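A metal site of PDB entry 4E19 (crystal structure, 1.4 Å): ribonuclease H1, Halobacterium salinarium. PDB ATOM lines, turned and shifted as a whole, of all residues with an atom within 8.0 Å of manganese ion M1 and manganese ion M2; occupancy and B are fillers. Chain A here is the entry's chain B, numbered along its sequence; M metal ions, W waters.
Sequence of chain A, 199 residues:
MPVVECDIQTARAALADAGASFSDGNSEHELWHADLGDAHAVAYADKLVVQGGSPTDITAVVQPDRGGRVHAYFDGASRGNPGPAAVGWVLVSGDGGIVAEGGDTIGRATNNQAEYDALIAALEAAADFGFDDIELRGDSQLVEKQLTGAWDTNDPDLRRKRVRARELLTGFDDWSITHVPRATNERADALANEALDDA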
ATOM      1  N   PHE A  74      24.779 -15.775  25.793  1.00  0.00           N
ATOM      2  CA  PHE A  74      23.684 -15.140  26.533  1.00  0.00           C
ATOM      3  C   PHE A  74      23.997 -13.657  26.640  1.00  0.00           C
ATOM      4  O   PHE A  74      25.201 -13.271  26.709  1.00  0.00           O
ATOM      5  CB  PHE A  74      23.570 -15.781  27.956  1.00  0.00           C
ATOM      6  CG  PHE A  74      24.788 -15.603  28.830  1.00  0.00           C
ATOM      7  CD1 PHE A  74      24.792 -14.565  29.758  1.00  0.00           C
ATOM      8  CD2 PHE A  74      25.821 -16.507  28.785  1.00  0.00           C
ATOM      9  CE1 PHE A  74      25.942 -14.377  30.608  1.00  0.00           C
ATOM     10  CE2 PHE A  74      26.972 -16.266  29.602  1.00  0.00           C
ATOM     11  CZ  PHE A  74      26.952 -15.248  30.532  1.00  0.00           C
ATOM     12  N   ASP A  75      22.970 -12.865  26.708  1.00  0.00           N
ATOM     13  CA  ASP A  75      23.094 -11.446  26.871  1.00  0.00           C
ATOM     14  C   ASP A  75      21.887 -10.820  27.416  1.00  0.00           C
ATOM     15  O   ASP A  75      20.772 -11.199  27.029  1.00  0.00           O
ATOM     16  CB  ASP A  75      23.476 -10.718  25.552  1.00  0.00           C
ATOM     17  CG  ASP A  75      24.270  -9.440  25.800  1.00  0.00           C
ATOM     18  OD1 ASP A  75      25.194  -9.497  26.627  1.00  0.00           O
ATOM     19  OD2 ASP A  75      23.925  -8.458  25.170  1.00  0.00           O
ATOM     20  N   GLY A  76      22.047  -9.909  28.380  1.00  0.00           N
ATOM     21  CA  GLY A  76      20.873  -9.158  28.900  1.00  0.00           C
ATOM     22  C   GLY A  76      20.834  -7.764  28.351  1.00  0.00           C
ATOM     23  O   GLY A  76      21.916  -7.259  27.938  1.00  0.00           O
ATOM     24  N   ALA A  77      19.716  -7.084  28.486  1.00  0.00           N
ATOM     25  CA  ALA A  77      19.580  -5.677  28.099  1.00  0.00           C
ATOM     26  C   ALA A  77      18.653  -5.005  29.094  1.00  0.00           C
ATOM     27  O   ALA A  77      17.669  -5.503  29.420  1.00  0.00           O
ATOM     28  CB  ALA A  77      19.008  -5.580  26.723  1.00  0.00           C
ATOM     29  N   SER A  78      19.065  -3.845  29.586  1.00  0.00           N
ATOM     30  CA  SER A  78      18.268  -2.984  30.457  1.00  0.00           C
ATOM     31  C   SER A  78      18.241  -1.567  29.899  1.00  0.00           C
ATOM     32  O   SER A  78      19.225  -1.045  29.570  1.00  0.00           O
ATOM     33  CB  SER A  78      18.918  -2.987  31.834  1.00  0.00           C
ATOM     34  OG  SER A  78      18.353  -2.073  32.700  1.00  0.00           O
ATOM     35  N   ASN A 111      21.306  -3.675  34.580  1.00  0.00           N
ATOM     36  CA  ASN A 111      22.146  -4.347  33.559  1.00  0.00           C
ATOM     37  C   ASN A 111      22.612  -5.715  34.094  1.00  0.00           C
ATOM     38  O   ASN A 111      22.559  -6.742  33.388  1.00  0.00           O
ATOM     39  CB  ASN A 111      23.420  -3.510  33.276  1.00  0.00           C
ATOM     40  CG  ASN A 111      23.130  -2.148  32.635  1.00  0.00           C
ATOM     41  OD1 ASN A 111      22.161  -1.988  31.925  1.00  0.00           O
ATOM     42  ND2 ASN A 111      24.012  -1.160  32.927  1.00  0.00           N
ATOM     43  N   ALA A 114      19.781  -8.338  34.509  1.00  0.00           N
ATOM     44  CA  ALA A 114      19.369  -8.889  33.245  1.00  0.00           C
ATOM     45  C   ALA A 114      20.406  -9.836  32.623  1.00  0.00           C
ATOM     46  O   ALA A 114      20.062 -10.833  31.971  1.00  0.00           O
ATOM     47  CB  ALA A 114      19.101  -7.727  32.271  1.00  0.00           C
ATOM     48  N   GLU A 115      21.714  -9.497  32.818  1.00  0.00           N
ATOM     49  CA  GLU A 115      22.730 -10.384  32.300  1.00  0.00           C
ATOM     50  C   GLU A 115      22.690 -11.786  32.959  1.00  0.00           C
ATOM     51  O   GLU A 115      22.814 -12.790  32.267  1.00  0.00           O
ATOM     52  CB  GLU A 115      24.111  -9.742  32.528  1.00  0.00           C
ATOM     53  CG  GLU A 115      25.205 -10.250  31.530  1.00  0.00           C
ATOM     54  CD  GLU A 115      25.141  -9.470  30.181  1.00  0.00           C
ATOM     55  OE1 GLU A 115      26.166  -9.545  29.462  1.00  0.00           O
ATOM     56  OE2 GLU A 115      24.133  -8.795  29.889  1.00  0.00           O
ATOM     57  N   ALA A 118      19.753 -13.655  31.707  1.00  0.00           N
ATOM     58  CA  ALA A 118      19.955 -14.231  30.380  1.00  0.00           C
ATOM     59  C   ALA A 118      20.762 -15.533  30.507  1.00  0.00           C
ATOM     60  O   ALA A 118      20.579 -16.492  29.777  1.00  0.00           O
ATOM     61  CB  ALA A 118      20.684 -13.238  29.490  1.00  0.00           C
ATOM     62  N   GLY A 138      29.776 -15.315  26.978  1.00  0.00           N
ATOM     63  CA  GLY A 138      29.182 -13.985  27.142  1.00  0.00           C
ATOM     64  C   GLY A 138      30.230 -12.892  27.254  1.00  0.00           C
ATOM     65  O   GLY A 138      31.416 -13.278  27.293  1.00  0.00           O
ATOM     66  N   ASP A 139      29.785 -11.637  27.254  1.00  0.00           N
ATOM     67  CA  ASP A 139      30.702 -10.553  27.148  1.00  0.00           C
ATOM     68  C   ASP A 139      30.741  -9.746  28.439  1.00  0.00           C
ATOM     69  O   ASP A 139      31.260  -8.593  28.454  1.00  0.00           O
ATOM     70  CB  ASP A 139      30.321  -9.629  25.959  1.00  0.00           C
ATOM     71  CG  ASP A 139      28.904  -9.158  26.002  1.00  0.00           C
ATOM     72  OD1 ASP A 139      28.329  -9.155  27.093  1.00  0.00           O
ATOM     73  OD2 ASP A 139      28.393  -8.671  24.990  1.00  0.00           O
ATOM     74  N   SER A 140      30.288 -10.335  29.564  1.00  0.00           N
ATOM     75  CA  SER A 140      30.400  -9.613  30.865  1.00  0.00           C
ATOM     76  C   SER A 140      31.301 -10.378  31.797  1.00  0.00           C
ATOM     77  O   SER A 140      31.041 -11.485  32.311  1.00  0.00           O
ATOM     78  CB  SER A 140      29.002  -9.552  31.503  1.00  0.00           C
ATOM     79  OG  SER A 140      29.116  -9.041  32.873  1.00  0.00           O
ATOM     80  N   GLN A 141      32.506  -9.808  32.016  1.00  0.00           N
ATOM     81  CA  GLN A 141      33.401 -10.396  33.023  1.00  0.00           C
ATOM     82  C   GLN A 141      32.836 -10.286  34.380  1.00  0.00           C
ATOM     83  O   GLN A 141      33.144 -11.172  35.249  1.00  0.00           O
ATOM     84  CB  GLN A 141      34.748  -9.633  32.933  1.00  0.00           C
ATOM     85  CG  GLN A 141      35.565 -10.127  31.727  1.00  0.00           C
ATOM     86  CD  GLN A 141      36.807  -9.344  31.678  1.00  0.00           C
ATOM     87  OE1 GLN A 141      36.800  -8.143  31.390  1.00  0.00           O
ATOM     88  NE2 GLN A 141      37.909  -9.984  32.054  1.00  0.00           N
ATOM     89  N   VAL A 143      29.723 -10.939  35.392  1.00  0.00           N
ATOM     90  CA  VAL A 143      28.981 -12.126  35.640  1.00  0.00           C
ATOM     91  C   VAL A 143      29.875 -13.372  35.595  1.00  0.00           C
ATOM     92  O   VAL A 143      29.807 -14.285  36.451  1.00  0.00           O
ATOM     93  CB  VAL A 143      27.880 -12.301  34.564  1.00  0.00           C
ATOM     94  CG1 VAL A 143      27.270 -13.743  34.664  1.00  0.00           C
ATOM     95  CG2 VAL A 143      26.807 -11.217  34.756  1.00  0.00           C
ATOM     96  N   VAL A 180      33.804 -13.647  25.639  1.00  0.00           N
ATOM     97  CA  VAL A 180      33.950 -13.263  24.228  1.00  0.00           C
ATOM     98  C   VAL A 180      33.754 -11.778  24.220  1.00  0.00           C
ATOM     99  O   VAL A 180      33.028 -11.194  25.044  1.00  0.00           O
ATOM    100  CB  VAL A 180      32.919 -13.944  23.336  1.00  0.00           C
ATOM    101  CG1 VAL A 180      33.112 -15.455  23.296  1.00  0.00           C
ATOM    102  CG2 VAL A 180      31.445 -13.563  23.676  1.00  0.00           C
ATOM    103  N   ARG A 182      32.279  -8.097  23.086  1.00  0.00           N
ATOM    104  CA  ARG A 182      30.948  -7.564  22.713  1.00  0.00           C
ATOM    105  C   ARG A 182      30.562  -7.883  21.277  1.00  0.00           C
ATOM    106  O   ARG A 182      29.447  -8.335  21.050  1.00  0.00           O
ATOM    107  CB  ARG A 182      30.943  -6.054  23.001  1.00  0.00           C
ATOM    108  CG  ARG A 182      29.815  -5.284  22.382  1.00  0.00           C
ATOM    109  CD  ARG A 182      28.404  -5.611  23.004  1.00  0.00           C
ATOM    110  NE  ARG A 182      27.397  -4.877  22.283  1.00  0.00           N
ATOM    111  CZ  ARG A 182      26.816  -5.300  21.141  1.00  0.00           C
ATOM    112  NH1 ARG A 182      25.931  -4.564  20.500  1.00  0.00           N
ATOM    113  NH2 ARG A 182      27.177  -6.464  20.656  1.00  0.00           N
ATOM    114  N   ASN A 185      29.387 -11.331  20.653  1.00  0.00           N
ATOM    115  CA  ASN A 185      28.089 -11.647  21.305  1.00  0.00           C
ATOM    116  C   ASN A 185      26.972 -10.823  20.732  1.00  0.00           C
ATOM    117  O   ASN A 185      25.895 -10.680  21.360  1.00  0.00           O
ATOM    118  CB  ASN A 185      28.246 -11.404  22.800  1.00  0.00           C
ATOM    119  CG  ASN A 185      27.183 -12.159  23.593  1.00  0.00           C
ATOM    120  OD1 ASN A 185      26.762 -13.224  23.226  1.00  0.00           O
ATOM    121  ND2 ASN A 185      26.802 -11.609  24.769  1.00  0.00           N
ATOM    122  N   GLU A 186      27.117 -10.368  19.478  1.00  0.00           N
ATOM    123  CA  GLU A 186      26.117  -9.546  18.883  1.00  0.00           C
ATOM    124  C   GLU A 186      24.721 -10.268  18.712  1.00  0.00           C
ATOM    125  O   GLU A 186      23.695  -9.564  18.835  1.00  0.00           O
ATOM    126  CB  GLU A 186      26.610  -9.091  17.468  1.00  0.00           C
ATOM    127  CG  GLU A 186      25.572  -8.283  16.638  1.00  0.00           C
ATOM    128  CD  GLU A 186      25.039  -7.003  17.314  1.00  0.00           C
ATOM    129  OE1 GLU A 186      25.736  -6.416  18.191  1.00  0.00           O
ATOM    130  OE2 GLU A 186      23.911  -6.561  17.001  1.00  0.00           O
ATOM    131  N   ALA A 188      23.105 -12.591  20.542  1.00  0.00           N
ATOM    132  CA  ALA A 188      22.293 -12.503  21.751  1.00  0.00           C
ATOM    133  C   ALA A 188      21.941 -11.088  22.196  1.00  0.00           C
ATOM    134  O   ALA A 188      20.835 -10.839  22.670  1.00  0.00           O
ATOM    135  CB  ALA A 188      23.014 -13.277  22.873  1.00  0.00           C
ATOM    136  N   ASP A 189      22.924 -10.164  22.007  1.00  0.00           N
ATOM    137  CA  ASP A 189      22.657  -8.762  22.297  1.00  0.00           C
ATOM    138  C   ASP A 189      21.515  -8.170  21.441  1.00  0.00           C
ATOM    139  O   ASP A 189      20.556  -7.642  21.982  1.00  0.00           O
ATOM    140  CB  ASP A 189      23.930  -7.979  22.047  1.00  0.00           C
ATOM    141  CG  ASP A 189      23.777  -6.544  22.291  1.00  0.00           C
ATOM    142  OD1 ASP A 189      24.451  -6.023  23.313  1.00  0.00           O
ATOM    143  OD2 ASP A 189      23.000  -5.788  21.610  1.00  0.00           O
ATOM    144  N   ALA A 190      21.519  -8.605  20.164  1.00  0.00           N
ATOM    145  CA  ALA A 190      20.415  -8.110  19.286  1.00  0.00           C
ATOM    146  C   ALA A 190      19.090  -8.770  19.649  1.00  0.00           C
ATOM    147  O   ALA A 190      18.023  -8.114  19.595  1.00  0.00           O
ATOM    148  CB  ALA A 190      20.812  -8.351  17.823  1.00  0.00           C
ATOM    149  N   ALA A 192      18.068  -9.665  22.680  1.00  0.00           N
ATOM    150  CA  ALA A 192      17.501  -8.971  23.822  1.00  0.00           C
ATOM    151  C   ALA A 192      16.959  -7.586  23.444  1.00  0.00           C
ATOM    152  O   ALA A 192      15.839  -7.228  23.893  1.00  0.00           O
ATOM    153  CB  ALA A 192      18.609  -8.879  24.889  1.00  0.00           C
ATOM    154  N   ASN A 193      17.769  -6.845  22.749  1.00  0.00           N
ATOM    155  CA  ASN A 193      17.313  -5.497  22.370  1.00  0.00           C
ATOM    156  C   ASN A 193      16.075  -5.525  21.443  1.00  0.00           C
ATOM    157  O   ASN A 193      15.194  -4.727  21.636  1.00  0.00           O
ATOM    158  CB  ASN A 193      18.434  -4.767  21.720  1.00  0.00           C
ATOM    159  CG  ASN A 193      19.356  -4.143  22.775  1.00  0.00           C
ATOM    160  OD1 ASN A 193      18.970  -3.192  23.521  1.00  0.00           O
ATOM    161  ND2 ASN A 193      20.479  -4.804  22.997  1.00  0.00           N
HETATM  162 MN    MN M   1      26.422  -8.254  27.772  1.00  0.00          MN
HETATM  163 MN    MN M   2      24.622  -6.395  25.350  1.00  0.00          MN
HETATM  164  O   HOH W   1      22.516  -5.773  25.699  1.00  0.00           O
HETATM  165  O   HOH W   2      27.414  -6.893  28.990  1.00  0.00           O
HETATM  166  O   HOH W   3      26.773  -6.934  25.790  1.00  0.00           O
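The side-chain carboxylate (OD2) of Asp 189 lies within salt-bridge range of the guanidinium group (NH1) of Arg 182 (3.4 Å).
The backbone NH (N) of Gly 76 sits at hydrogen-bond distance from the side-chain carboxylate (OE2) of Glu 115.
ND2 of Asn 193 lies within hydrogen-bond range of O of Asp 189.
OD2 of Asp 139 sits at hydrogen-bond distance from ND2 of Asn 185 (3.3 Å).
OD1 of Asp 75 sits close to ND2 of Asn 185 (3.2 Å).
Three residues have an atom within 4 Å of manganese ion M1: Asp 75, Glu 115 and Asp 139.
Along chain A the residues within 4 Å of manganese ion M1 span positions 75 to 139.
Merely in contact with manganese ion M2: Gly 76.
Manganese ion M1 is bound by water W2 (2.1 Å), OD1 of Asp 75 (2.1 Å), OE1 of Glu 115 (2.1 Å), OD1 of Asp 139 (2.2 Å) and water W3 (2.4 Å).
Manganese ion M2 is bound by the side-chain carboxylate (OD1) of Asp 189, 2.1 Å away.
The side-chain carboxylate (OD2) of Asp 75 is bound to manganese ion M2.
Water W1 binds manganese ion M2, at 2.2 Å.
Manganese ion M2 is bound by water W3, at 2.3 Å.
Manganese ion M2 has four donor atoms within binding distance.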
